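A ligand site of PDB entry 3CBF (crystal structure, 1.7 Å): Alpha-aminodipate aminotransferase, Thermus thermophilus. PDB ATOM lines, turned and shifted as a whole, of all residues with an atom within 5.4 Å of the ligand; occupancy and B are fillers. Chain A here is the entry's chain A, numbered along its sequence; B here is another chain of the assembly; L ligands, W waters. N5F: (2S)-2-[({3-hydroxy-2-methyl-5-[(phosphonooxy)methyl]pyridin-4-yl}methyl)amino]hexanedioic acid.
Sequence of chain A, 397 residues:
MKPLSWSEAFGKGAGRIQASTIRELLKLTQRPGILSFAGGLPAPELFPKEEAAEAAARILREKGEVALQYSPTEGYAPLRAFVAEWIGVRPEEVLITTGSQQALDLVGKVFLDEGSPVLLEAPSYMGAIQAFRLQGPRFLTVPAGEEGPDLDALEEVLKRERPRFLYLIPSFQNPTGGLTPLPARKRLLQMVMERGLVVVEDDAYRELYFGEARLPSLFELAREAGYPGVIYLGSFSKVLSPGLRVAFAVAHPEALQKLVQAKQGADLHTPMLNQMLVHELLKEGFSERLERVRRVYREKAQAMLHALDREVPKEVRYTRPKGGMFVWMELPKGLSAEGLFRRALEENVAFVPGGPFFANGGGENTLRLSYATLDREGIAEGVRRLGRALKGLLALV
OAN of the ligand sits at hydrogen-bond distance from OH of Tyr 205 (2.6 Å). An oxygen (OAM) of the ligand is in hydrogen-bond range of the side-chain hydroxyl of Ser 237. The side-chain hydroxyl (OH) of Tyr 70 of chain B lies within hydrogen-bond range of an oxygen (OAM) of the ligand (2.6 Å). N of Ser 100 lies within hydrogen-bond range of OAZ of the ligand, at 2.8 Å. OAZ of the ligand lies within hydrogen-bond range of OG of Ser 100 (2.6 Å). The side-chain hydroxyl (OG) of Ser 235 sits at hydrogen-bond distance from an oxygen (OAZ) of the ligand (2.7 Å). A nitrogen (NAX) of the ligand is in hydrogen-bond range of the side-chain carboxylate (OD2) of Asp 202 (2.7 Å). OAU of the ligand lies within salt-bridge range of NH2 of Arg 245 (2.7 Å). N of Gly 40 is in hydrogen-bond range of O of the ligand, at 2.7 Å. The side-chain amide nitrogen of Asn 174 sits at hydrogen-bond distance from an oxygen (OAN) of the ligand, 2.8 Å away. NH1 of Arg 23 lies within salt-bridge range of OAB of the ligand (2.8 Å). An oxygen (OXT) of the ligand is in salt-bridge range of the guanidinium group (NH1) of Arg 368 (2.9 Å). N of Gln 101 sits at hydrogen-bond distance from OAU of the ligand, at 2.9 Å. A nitrogen (N) of the ligand sits close to the side-chain amino group of Lys 238 (3.2 Å).
OG of Ser 235 sits at hydrogen-bond distance from N of Ser 237 (3.0 Å). The backbone NH (N) of Gly 99 lies within hydrogen-bond range of the backbone carbonyl oxygen (O) of Arg 245 (3.5 Å). O of Pro 242 lies within hydrogen-bond range of NH1 of Arg 245 (3.1 Å). The guanidinium group of Arg 245 sits at hydrogen-bond distance from the backbone carbonyl oxygen of Asp 267 of chain B. NH1 of Arg 368 sits at hydrogen-bond distance from OD1 of Asn 174 (3.0 Å). The backbone NH of Tyr 125 lies within hydrogen-bond range of the backbone carbonyl oxygen of Asn 174 (3.2 Å). The backbone carbonyl oxygen (O) of Leu 268 of chain B lies within hydrogen-bond range of the guanidinium group (NH2) of Arg 23, 3.4 Å away. NE2 of Gln 101 lies within hydrogen-bond range of OH of Tyr 125 (3.0 Å).
Residues that only touch the ligand: Ile 22 (3.4 Å), Leu 26 (3.8 Å), Gly 39 (3.6 Å), Gly 99 (3.4 Å), Tyr 125 (3.4 Å), Tyr 167 (3.8 Å), Ile 169 (3.7 Å), Phe 326 (3.9 Å) and Leu 268 of chain B (3.8 Å). Hydrophobic or aromatic side chains within 4 Å of the ligand: Ile 22, Leu 26, Tyr 125, Ile 169, Tyr 205, Phe 326, Tyr 70 of chain B and Leu 268 of chain B. 22 residues have an atom within 4 Å of the ligand: Ile 22, Arg 23, Leu 26, Gly 39, Gly 40, Gly 99, Ser 100, Gln 101, Tyr 125, Tyr 167, Ile 169, Asn 174, Asp 202, Tyr 205, Ser 235, Ser 237, Lys 238, Arg 245, Phe 326, Arg 368, Tyr 70 of chain B and Leu 268 of chain B. The nearest printed residue that does not touch the ligand is Ala 204 (4.05 Å).
Water W2 lies within hydrogen-bond range of OAJ of the ligand (2.6 Å) and OH of Tyr 125 (3.0 Å). Water W1 bridges the backbone carbonyl oxygen of Ile 22 (2.8 Å) and an oxygen (OAB) of the ligand (2.8 Å).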
ATOM      1  N   ILE A  22      24.750 -12.215  -7.755  1.00  0.00           N
ATOM      2  CA  ILE A  22      23.418 -11.870  -8.221  1.00  0.00           C
ATOM      3  C   ILE A  22      23.357 -11.970  -9.732  1.00  0.00           C
ATOM      4  O   ILE A  22      22.399 -12.532 -10.304  1.00  0.00           O
ATOM      5  CB  ILE A  22      22.937 -10.464  -7.760  1.00  0.00           C
ATOM      6  CG1 ILE A  22      22.764 -10.393  -6.243  1.00  0.00           C
ATOM      7  CG2 ILE A  22      21.601 -10.157  -8.414  1.00  0.00           C
ATOM      8  CD1 ILE A  22      22.540  -8.959  -5.708  1.00  0.00           C
ATOM      9  N   ARG A  23      24.364 -11.413 -10.396  1.00  0.00           N
ATOM     10  CA  ARG A  23      24.312 -11.348 -11.865  1.00  0.00           C
ATOM     11  C   ARG A  23      24.403 -12.757 -12.433  1.00  0.00           C
ATOM     12  O   ARG A  23      23.697 -13.108 -13.384  1.00  0.00           O
ATOM     13  CB  ARG A  23      25.478 -10.516 -12.400  1.00  0.00           C
ATOM     14  CG  ARG A  23      25.392  -9.000 -12.132  1.00  0.00           C
ATOM     15  CD  ARG A  23      24.739  -8.310 -13.329  1.00  0.00           C
ATOM     16  NE  ARG A  23      23.288  -8.500 -13.363  1.00  0.00           N
ATOM     17  CZ  ARG A  23      22.579  -8.712 -14.466  1.00  0.00           C
ATOM     18  NH1 ARG A  23      21.264  -8.838 -14.404  1.00  0.00           N
ATOM     19  NH2 ARG A  23      23.181  -8.816 -15.662  1.00  0.00           N
ATOM     20  N   LEU A  26      21.119 -15.114 -12.149  1.00  0.00           N
ATOM     21  CA  LEU A  26      20.030 -14.900 -13.113  1.00  0.00           C
ATOM     22  C   LEU A  26      20.032 -15.915 -14.256  1.00  0.00           C
ATOM     23  O   LEU A  26      18.974 -16.235 -14.806  1.00  0.00           O
ATOM     24  CB  LEU A  26      20.113 -13.468 -13.679  1.00  0.00           C
ATOM     25  CG  LEU A  26      18.972 -12.986 -14.590  1.00  0.00           C
ATOM     26  CD1 LEU A  26      17.607 -13.193 -13.935  1.00  0.00           C
ATOM     27  CD2 LEU A  26      19.158 -11.543 -14.937  1.00  0.00           C
ATOM     28  N   ALA A  38      16.085 -15.041  -5.469  1.00  0.00           N
ATOM     29  CA  ALA A  38      17.469 -14.588  -5.673  1.00  0.00           C
ATOM     30  C   ALA A  38      17.444 -13.111  -6.061  1.00  0.00           C
ATOM     31  O   ALA A  38      17.138 -12.263  -5.229  1.00  0.00           O
ATOM     32  CB  ALA A  38      18.167 -15.440  -6.737  1.00  0.00           C
ATOM     33  N   GLY A  39      17.746 -12.788  -7.314  1.00  0.00           N
ATOM     34  CA  GLY A  39      17.760 -11.397  -7.738  1.00  0.00           C
ATOM     35  C   GLY A  39      16.426 -10.724  -7.490  1.00  0.00           C
ATOM     36  O   GLY A  39      15.356 -11.326  -7.705  1.00  0.00           O
ATOM     37  N   GLY A  40      16.495  -9.464  -7.057  1.00  0.00           N
ATOM     38  CA  GLY A  40      15.285  -8.645  -6.861  1.00  0.00           C
ATOM     39  C   GLY A  40      14.614  -8.260  -8.165  1.00  0.00           C
ATOM     40  O   GLY A  40      14.556  -7.092  -8.517  1.00  0.00           O
ATOM     41  N   LEU A  41      14.065  -9.254  -8.865  1.00  0.00           N
ATOM     42  CA  LEU A  41      13.434  -9.047 -10.155  1.00  0.00           C
ATOM     43  C   LEU A  41      11.962  -8.736  -9.941  1.00  0.00           C
ATOM     44  O   LEU A  41      11.250  -9.541  -9.313  1.00  0.00           O
ATOM     45  CB  LEU A  41      13.620 -10.268 -11.050  1.00  0.00           C
ATOM     46  CG  LEU A  41      14.834 -10.209 -12.002  1.00  0.00           C
ATOM     47  CD1 LEU A  41      16.124 -10.356 -11.212  1.00  0.00           C
ATOM     48  CD2 LEU A  41      14.737 -11.327 -13.002  1.00  0.00           C
ATOM     49  N   THR A  98      22.310   4.916 -17.011  1.00  0.00           N
ATOM     50  CA  THR A  98      21.931   3.632 -17.625  1.00  0.00           C
ATOM     51  C   THR A  98      21.736   2.628 -16.486  1.00  0.00           C
ATOM     52  O   THR A  98      22.549   1.715 -16.269  1.00  0.00           O
ATOM     53  CB  THR A  98      22.967   3.196 -18.686  1.00  0.00           C
ATOM     54  OG1 THR A  98      23.094   4.230 -19.654  1.00  0.00           O
ATOM     55  CG2 THR A  98      22.542   1.903 -19.400  1.00  0.00           C
ATOM     56  N   GLY A  99      20.679   2.874 -15.703  1.00  0.00           N
ATOM     57  CA  GLY A  99      20.436   2.186 -14.442  1.00  0.00           C
ATOM     58  C   GLY A  99      21.246   2.873 -13.355  1.00  0.00           C
ATOM     59  O   GLY A  99      22.176   3.611 -13.673  1.00  0.00           O
ATOM     60  N   SER A 100      20.854   2.674 -12.103  1.00  0.00           N
ATOM     61  CA  SER A 100      21.574   3.324 -10.997  1.00  0.00           C
ATOM     62  C   SER A 100      22.881   2.577 -10.832  1.00  0.00           C
ATOM     63  O   SER A 100      23.864   3.114 -10.240  1.00  0.00           O
ATOM     64  CB  SER A 100      20.747   3.429  -9.694  1.00  0.00           C
ATOM     65  OG  SER A 100      20.278   2.163  -9.263  1.00  0.00           O
ATOM     66  N   GLN A 101      22.946   1.344 -11.339  1.00  0.00           N
ATOM     67  CA  GLN A 101      24.256   0.653 -11.365  1.00  0.00           C
ATOM     68  C   GLN A 101      25.350   1.538 -12.020  1.00  0.00           C
ATOM     69  O   GLN A 101      26.482   1.625 -11.526  1.00  0.00           O
ATOM     70  CB  GLN A 101      24.210  -0.699 -12.084  1.00  0.00           C
ATOM     71  CG  GLN A 101      25.547  -1.479 -11.986  1.00  0.00           C
ATOM     72  CD  GLN A 101      26.001  -1.743 -10.543  1.00  0.00           C
ATOM     73  OE1 GLN A 101      27.212  -1.612 -10.209  1.00  0.00           O
ATOM     74  NE2 GLN A 101      25.081  -2.151  -9.711  1.00  0.00           N
ATOM     75  N   GLN A 102      25.018   2.186 -13.127  1.00  0.00           N
ATOM     76  CA  GLN A 102      25.977   3.125 -13.738  1.00  0.00           C
ATOM     77  C   GLN A 102      26.356   4.240 -12.803  1.00  0.00           C
ATOM     78  O   GLN A 102      27.549   4.579 -12.684  1.00  0.00           O
ATOM     79  CB  GLN A 102      25.404   3.698 -15.017  1.00  0.00           C
ATOM     80  CG  GLN A 102      26.386   4.686 -15.674  1.00  0.00           C
ATOM     81  CD  GLN A 102      25.980   5.015 -17.068  1.00  0.00           C
ATOM     82  OE1 GLN A 102      25.075   5.793 -17.249  1.00  0.00           O
ATOM     83  NE2 GLN A 102      26.687   4.464 -18.047  1.00  0.00           N
ATOM     84  N   LEU A 104      26.628   4.173  -9.686  1.00  0.00           N
ATOM     85  CA  LEU A 104      27.611   3.622  -8.733  1.00  0.00           C
ATOM     86  C   LEU A 104      28.983   3.556  -9.384  1.00  0.00           C
ATOM     87  O   LEU A 104      29.979   3.913  -8.752  1.00  0.00           O
ATOM     88  CB  LEU A 104      27.184   2.209  -8.276  1.00  0.00           C
ATOM     89  CG  LEU A 104      25.764   2.155  -7.665  1.00  0.00           C
ATOM     90  CD1 LEU A 104      25.365   0.702  -7.310  1.00  0.00           C
ATOM     91  CD2 LEU A 104      25.702   3.047  -6.445  1.00  0.00           C
ATOM     92  N   TYR A 125      24.982  -3.434  -0.595  1.00  0.00           N
ATOM     93  CA  TYR A 125      24.642  -3.916  -1.937  1.00  0.00           C
ATOM     94  C   TYR A 125      25.895  -4.383  -2.689  1.00  0.00           C
ATOM     95  O   TYR A 125      26.849  -3.603  -2.875  1.00  0.00           O
ATOM     96  CB  TYR A 125      23.929  -2.800  -2.689  1.00  0.00           C
ATOM     97  CG  TYR A 125      23.703  -3.099  -4.171  1.00  0.00           C
ATOM     98  CD1 TYR A 125      23.164  -4.328  -4.598  1.00  0.00           C
ATOM     99  CD2 TYR A 125      24.033  -2.155  -5.135  1.00  0.00           C
ATOM    100  CE1 TYR A 125      22.959  -4.590  -5.941  1.00  0.00           C
ATOM    101  CE2 TYR A 125      23.840  -2.397  -6.482  1.00  0.00           C
ATOM    102  CZ  TYR A 125      23.299  -3.615  -6.888  1.00  0.00           C
ATOM    103  OH  TYR A 125      23.145  -3.820  -8.227  1.00  0.00           O
ATOM    104  N   TYR A 167      28.557   5.465   1.464  1.00  0.00           N
ATOM    105  CA  TYR A 167      27.513   4.903   0.624  1.00  0.00           C
ATOM    106  C   TYR A 167      26.402   4.279   1.513  1.00  0.00           C
ATOM    107  O   TYR A 167      26.670   3.331   2.269  1.00  0.00           O
ATOM    108  CB  TYR A 167      28.080   3.840  -0.347  1.00  0.00           C
ATOM    109  CG  TYR A 167      26.976   3.089  -1.122  1.00  0.00           C
ATOM    110  CD1 TYR A 167      26.279   3.710  -2.134  1.00  0.00           C
ATOM    111  CD2 TYR A 167      26.632   1.753  -0.797  1.00  0.00           C
ATOM    112  CE1 TYR A 167      25.273   3.025  -2.847  1.00  0.00           C
ATOM    113  CE2 TYR A 167      25.607   1.063  -1.495  1.00  0.00           C
ATOM    114  CZ  TYR A 167      24.946   1.703  -2.513  1.00  0.00           C
ATOM    115  OH  TYR A 167      23.928   0.998  -3.221  1.00  0.00           O
ATOM    116  N   ILE A 169      21.969   3.208   2.047  1.00  0.00           N
ATOM    117  CA  ILE A 169      20.669   2.910   1.431  1.00  0.00           C
ATOM    118  C   ILE A 169      19.617   2.996   2.545  1.00  0.00           C
ATOM    119  O   ILE A 169      19.196   1.973   3.061  1.00  0.00           O
ATOM    120  CB  ILE A 169      20.630   1.503   0.727  1.00  0.00           C
ATOM    121  CG1 ILE A 169      21.814   1.310  -0.240  1.00  0.00           C
ATOM    122  CG2 ILE A 169      19.261   1.307  -0.023  1.00  0.00           C
ATOM    123  CD1 ILE A 169      22.187  -0.184  -0.466  1.00  0.00           C
ATOM    124  N   ASN A 174      19.374  -2.842   0.821  1.00  0.00           N
ATOM    125  CA  ASN A 174      19.834  -4.083   0.235  1.00  0.00           C
ATOM    126  C   ASN A 174      21.157  -4.463   0.920  1.00  0.00           C
ATOM    127  O   ASN A 174      22.127  -3.737   0.794  1.00  0.00           O
ATOM    128  CB  ASN A 174      20.027  -3.862  -1.256  1.00  0.00           C
ATOM    129  CG  ASN A 174      20.384  -5.126  -2.000  1.00  0.00           C
ATOM    130  OD1 ASN A 174      20.603  -6.186  -1.404  1.00  0.00           O
ATOM    131  ND2 ASN A 174      20.398  -5.029  -3.309  1.00  0.00           N
ATOM    132  N   ASP A 202      21.519   5.895  -2.021  1.00  0.00           N
ATOM    133  CA  ASP A 202      20.973   5.070  -3.084  1.00  0.00           C
ATOM    134  C   ASP A 202      19.527   4.834  -2.705  1.00  0.00           C
ATOM    135  O   ASP A 202      19.244   4.086  -1.766  1.00  0.00           O
ATOM    136  CB  ASP A 202      21.793   3.781  -3.187  1.00  0.00           C
ATOM    137  CG  ASP A 202      21.360   2.882  -4.336  1.00  0.00           C
ATOM    138  OD1 ASP A 202      20.197   2.976  -4.781  1.00  0.00           O
ATOM    139  OD2 ASP A 202      22.205   2.069  -4.802  1.00  0.00           O
ATOM    140  N   ALA A 204      16.955   3.340  -4.426  1.00  0.00           N
ATOM    141  CA  ALA A 204      16.309   2.476  -5.433  1.00  0.00           C
ATOM    142  C   ALA A 204      14.873   2.066  -5.026  1.00  0.00           C
ATOM    143  O   ALA A 204      13.988   1.886  -5.873  1.00  0.00           O
ATOM    144  CB  ALA A 204      17.161   1.235  -5.676  1.00  0.00           C
ATOM    145  N   TYR A 205      14.676   1.915  -3.716  1.00  0.00           N
ATOM    146  CA  TYR A 205      13.435   1.396  -3.115  1.00  0.00           C
ATOM    147  C   TYR A 205      12.544   2.488  -2.527  1.00  0.00           C
ATOM    148  O   TYR A 205      11.621   2.167  -1.779  1.00  0.00           O
ATOM    149  CB  TYR A 205      13.795   0.334  -2.043  1.00  0.00           C
ATOM    150  CG  TYR A 205      14.622  -0.754  -2.661  1.00  0.00           C
ATOM    151  CD1 TYR A 205      14.047  -1.703  -3.519  1.00  0.00           C
ATOM    152  CD2 TYR A 205      16.000  -0.788  -2.473  1.00  0.00           C
ATOM    153  CE1 TYR A 205      14.828  -2.678  -4.153  1.00  0.00           C
ATOM    154  CE2 TYR A 205      16.787  -1.755  -3.097  1.00  0.00           C
ATOM    155  CZ  TYR A 205      16.215  -2.695  -3.903  1.00  0.00           C
ATOM    156  OH  TYR A 205      17.041  -3.611  -4.521  1.00  0.00           O
ATOM    157  N   SER A 235      16.009   5.248  -9.410  1.00  0.00           N
ATOM    158  CA  SER A 235      15.911   4.353 -10.576  1.00  0.00           C
ATOM    159  C   SER A 235      14.461   4.104 -10.923  1.00  0.00           C
ATOM    160  O   SER A 235      13.587   4.108 -10.063  1.00  0.00           O
ATOM    161  CB  SER A 235      16.628   3.028 -10.301  1.00  0.00           C
ATOM    162  OG  SER A 235      16.580   2.149 -11.414  1.00  0.00           O
ATOM    163  N   SER A 237      13.869   1.237 -12.238  1.00  0.00           N
ATOM    164  CA  SER A 237      13.882  -0.217 -12.270  1.00  0.00           C
ATOM    165  C   SER A 237      12.814  -0.879 -11.389  1.00  0.00           C
ATOM    166  O   SER A 237      12.131  -1.815 -11.847  1.00  0.00           O
ATOM    167  CB  SER A 237      15.274  -0.765 -11.939  1.00  0.00           C
ATOM    168  OG  SER A 237      16.160  -0.458 -12.998  1.00  0.00           O
ATOM    169  N   LYS A 238      12.641  -0.412 -10.160  1.00  0.00           N
ATOM    170  CA  LYS A 238      11.744  -1.148  -9.264  1.00  0.00           C
ATOM    171  C   LYS A 238      10.314  -0.654  -9.365  1.00  0.00           C
ATOM    172  O   LYS A 238       9.396  -1.286  -8.843  1.00  0.00           O
ATOM    173  CB  LYS A 238      12.237  -1.116  -7.808  1.00  0.00           C
ATOM    174  CG  LYS A 238      13.683  -1.579  -7.602  1.00  0.00           C
ATOM    175  CD  LYS A 238      13.986  -2.928  -8.262  1.00  0.00           C
ATOM    176  CE  LYS A 238      15.280  -3.511  -7.718  1.00  0.00           C
ATOM    177  NZ  LYS A 238      16.506  -2.893  -8.287  1.00  0.00           N
ATOM    178  N   PRO A 242      13.087  -2.750 -15.009  1.00  0.00           N
ATOM    179  CA  PRO A 242      14.532  -2.836 -14.829  1.00  0.00           C
ATOM    180  C   PRO A 242      15.235  -3.013 -16.187  1.00  0.00           C
ATOM    181  O   PRO A 242      16.306  -2.448 -16.406  1.00  0.00           O
ATOM    182  CB  PRO A 242      14.711  -4.090 -13.939  1.00  0.00           C
ATOM    183  CG  PRO A 242      13.467  -4.823 -14.018  1.00  0.00           C
ATOM    184  CD  PRO A 242      12.379  -3.902 -14.442  1.00  0.00           C
ATOM    185  N   ARG A 245      16.759  -0.015 -18.271  1.00  0.00           N
ATOM    186  CA  ARG A 245      18.043   0.548 -17.821  1.00  0.00           C
ATOM    187  C   ARG A 245      17.990   2.086 -17.812  1.00  0.00           C
ATOM    188  O   ARG A 245      18.733   2.735 -18.551  1.00  0.00           O
ATOM    189  CB  ARG A 245      19.187   0.076 -18.703  1.00  0.00           C
ATOM    190  CG  ARG A 245      19.296  -1.430 -18.993  1.00  0.00           C
ATOM    191  CD  ARG A 245      19.416  -2.351 -17.748  1.00  0.00           C
ATOM    192  NE  ARG A 245      20.449  -1.965 -16.765  1.00  0.00           N
ATOM    193  CZ  ARG A 245      20.209  -1.660 -15.480  1.00  0.00           C
ATOM    194  NH1 ARG A 245      18.983  -1.657 -14.972  1.00  0.00           N
ATOM    195  NH2 ARG A 245      21.213  -1.354 -14.676  1.00  0.00           N
ATOM    196  N   ALA A 247      17.739   5.401 -15.072  1.00  0.00           N
ATOM    197  CA  ALA A 247      17.775   5.847 -13.722  1.00  0.00           C
ATOM    198  C   ALA A 247      18.314   7.281 -13.698  1.00  0.00           C
ATOM    199  O   ALA A 247      18.470   7.914 -14.743  1.00  0.00           O
ATOM    200  CB  ALA A 247      18.700   4.915 -12.959  1.00  0.00           C
ATOM    201  N   PHE A 326      13.291  -7.343   0.057  1.00  0.00           N
ATOM    202  CA  PHE A 326      14.137  -8.340   0.725  1.00  0.00           C
ATOM    203  C   PHE A 326      13.839  -8.691   2.194  1.00  0.00           C
ATOM    204  O   PHE A 326      13.436  -7.840   2.992  1.00  0.00           O
ATOM    205  CB  PHE A 326      15.611  -7.928   0.633  1.00  0.00           C
ATOM    206  CG  PHE A 326      16.051  -7.557  -0.746  1.00  0.00           C
ATOM    207  CD1 PHE A 326      16.019  -8.489  -1.781  1.00  0.00           C
ATOM    208  CD2 PHE A 326      16.464  -6.243  -1.026  1.00  0.00           C
ATOM    209  CE1 PHE A 326      16.425  -8.133  -3.078  1.00  0.00           C
ATOM    210  CE2 PHE A 326      16.858  -5.891  -2.304  1.00  0.00           C
ATOM    211  CZ  PHE A 326      16.851  -6.837  -3.339  1.00  0.00           C
ATOM    212  N   ARG A 368      20.224 -13.675   1.629  1.00  0.00           N
ATOM    213  CA  ARG A 368      19.165 -12.733   1.294  1.00  0.00           C
ATOM    214  C   ARG A 368      18.083 -13.463   0.519  1.00  0.00           C
ATOM    215  O   ARG A 368      18.395 -14.248  -0.370  1.00  0.00           O
ATOM    216  CB  ARG A 368      19.715 -11.575   0.440  1.00  0.00           C
ATOM    217  CG  ARG A 368      18.704 -10.443   0.175  1.00  0.00           C
ATOM    218  CD  ARG A 368      19.256  -9.520  -0.928  1.00  0.00           C
ATOM    219  NE  ARG A 368      19.097 -10.098  -2.270  1.00  0.00           N
ATOM    220  CZ  ARG A 368      19.474  -9.514  -3.408  1.00  0.00           C
ATOM    221  NH1 ARG A 368      20.011  -8.287  -3.415  1.00  0.00           N
ATOM    222  NH2 ARG A 368      19.255 -10.118  -4.564  1.00  0.00           N
ATOM    223  N   TYR B  70      15.220  -7.589 -15.983  1.00  0.00           N
ATOM    224  CA  TYR B  70      16.660  -7.823 -15.914  1.00  0.00           C
ATOM    225  C   TYR B  70      17.037  -9.069 -16.715  1.00  0.00           C
ATOM    226  O   TYR B  70      16.256 -10.007 -16.806  1.00  0.00           O
ATOM    227  CB  TYR B  70      17.103  -8.035 -14.460  1.00  0.00           C
ATOM    228  CG  TYR B  70      17.119  -6.823 -13.593  1.00  0.00           C
ATOM    229  CD1 TYR B  70      18.028  -5.781 -13.853  1.00  0.00           C
ATOM    230  CD2 TYR B  70      16.302  -6.732 -12.464  1.00  0.00           C
ATOM    231  CE1 TYR B  70      18.107  -4.683 -13.019  1.00  0.00           C
ATOM    232  CE2 TYR B  70      16.365  -5.633 -11.623  1.00  0.00           C
ATOM    233  CZ  TYR B  70      17.276  -4.602 -11.905  1.00  0.00           C
ATOM    234  OH  TYR B  70      17.373  -3.488 -11.105  1.00  0.00           O
ATOM    235  N   ASP B 267      26.978  -1.371 -15.719  1.00  0.00           N
ATOM    236  CA  ASP B 267      25.539  -1.099 -15.994  1.00  0.00           C
ATOM    237  C   ASP B 267      24.583  -2.302 -15.850  1.00  0.00           C
ATOM    238  O   ASP B 267      23.404  -2.235 -16.284  1.00  0.00           O
ATOM    239  CB  ASP B 267      25.351  -0.428 -17.369  1.00  0.00           C
ATOM    240  CG  ASP B 267      25.636  -1.362 -18.548  1.00  0.00           C
ATOM    241  OD1 ASP B 267      25.651  -0.840 -19.675  1.00  0.00           O
ATOM    242  OD2 ASP B 267      25.901  -2.588 -18.345  1.00  0.00           O
ATOM    243  N   LEU B 268      25.104  -3.372 -15.272  1.00  0.00           N
ATOM    244  CA  LEU B 268      24.452  -4.717 -15.212  1.00  0.00           C
ATOM    245  C   LEU B 268      24.385  -5.363 -16.603  1.00  0.00           C
ATOM    246  O   LEU B 268      25.113  -6.323 -16.888  1.00  0.00           O
ATOM    247  CB  LEU B 268      23.051  -4.698 -14.545  1.00  0.00           C
ATOM    248  CG  LEU B 268      22.957  -4.070 -13.155  1.00  0.00           C
ATOM    249  CD1 LEU B 268      21.545  -4.246 -12.583  1.00  0.00           C
ATOM    250  CD2 LEU B 268      24.038  -4.677 -12.224  1.00  0.00           C
HETATM  251  OAM N5F L   1      18.487  -1.391 -12.231  1.00  0.00           O
HETATM  252  PAT N5F L   1      19.514  -0.482 -11.505  1.00  0.00           P
HETATM  253  OAZ N5F L   1      18.914   0.916 -11.156  1.00  0.00           O
HETATM  254  OAU N5F L   1      20.845  -0.400 -12.224  1.00  0.00           O
HETATM  255  OAS N5F L   1      19.660  -1.304 -10.137  1.00  0.00           O
HETATM  256  CAR N5F L   1      20.922  -1.419  -9.462  1.00  0.00           C
HETATM  257  CAQ N5F L   1      20.741  -1.335  -7.951  1.00  0.00           C
HETATM  258  CAY N5F L   1      21.218  -0.177  -7.349  1.00  0.00           C
HETATM  259  NAX N5F L   1      21.089   0.001  -6.040  1.00  0.00           N
HETATM  260  CAW N5F L   1      20.569  -0.907  -5.230  1.00  0.00           C
HETATM  261  CAV N5F L   1      20.496  -0.607  -3.735  1.00  0.00           C
HETATM  262  CAO N5F L   1      20.080  -2.098  -5.767  1.00  0.00           C
HETATM  263  OAN N5F L   1      19.490  -2.997  -4.959  1.00  0.00           O
HETATM  264  CAP N5F L   1      20.137  -2.339  -7.165  1.00  0.00           C
HETATM  265  CAK N5F L   1      19.633  -3.652  -7.840  1.00  0.00           C
HETATM  266  N   N5F L   1      18.850  -4.484  -6.908  1.00  0.00           N
HETATM  267  CA  N5F L   1      18.432  -5.865  -7.244  1.00  0.00           C
HETATM  268  C   N5F L   1      19.187  -6.939  -6.450  1.00  0.00           C
HETATM  269  OXT N5F L   1      20.124  -6.568  -5.698  1.00  0.00           O
HETATM  270  O   N5F L   1      18.821  -8.122  -6.624  1.00  0.00           O
HETATM  271  CB  N5F L   1      18.282  -6.150  -8.758  1.00  0.00           C
HETATM  272  CAG N5F L   1      19.581  -6.661  -9.424  1.00  0.00           C
HETATM  273  CAH N5F L   1      19.216  -7.809 -10.378  1.00  0.00           C
HETATM  274  CAI N5F L   1      20.380  -8.341 -11.229  1.00  0.00           C
HETATM  275  OAB N5F L   1      20.102  -9.341 -11.933  1.00  0.00           O
HETATM  276  OAJ N5F L   1      21.497  -7.789 -11.127  1.00  0.00           O
HETATM  277  O   HOH W   1      19.699 -11.801 -10.566  1.00  0.00           O
HETATM  278  O   HOH W   2      22.805  -6.697  -9.098  1.00  0.00           O
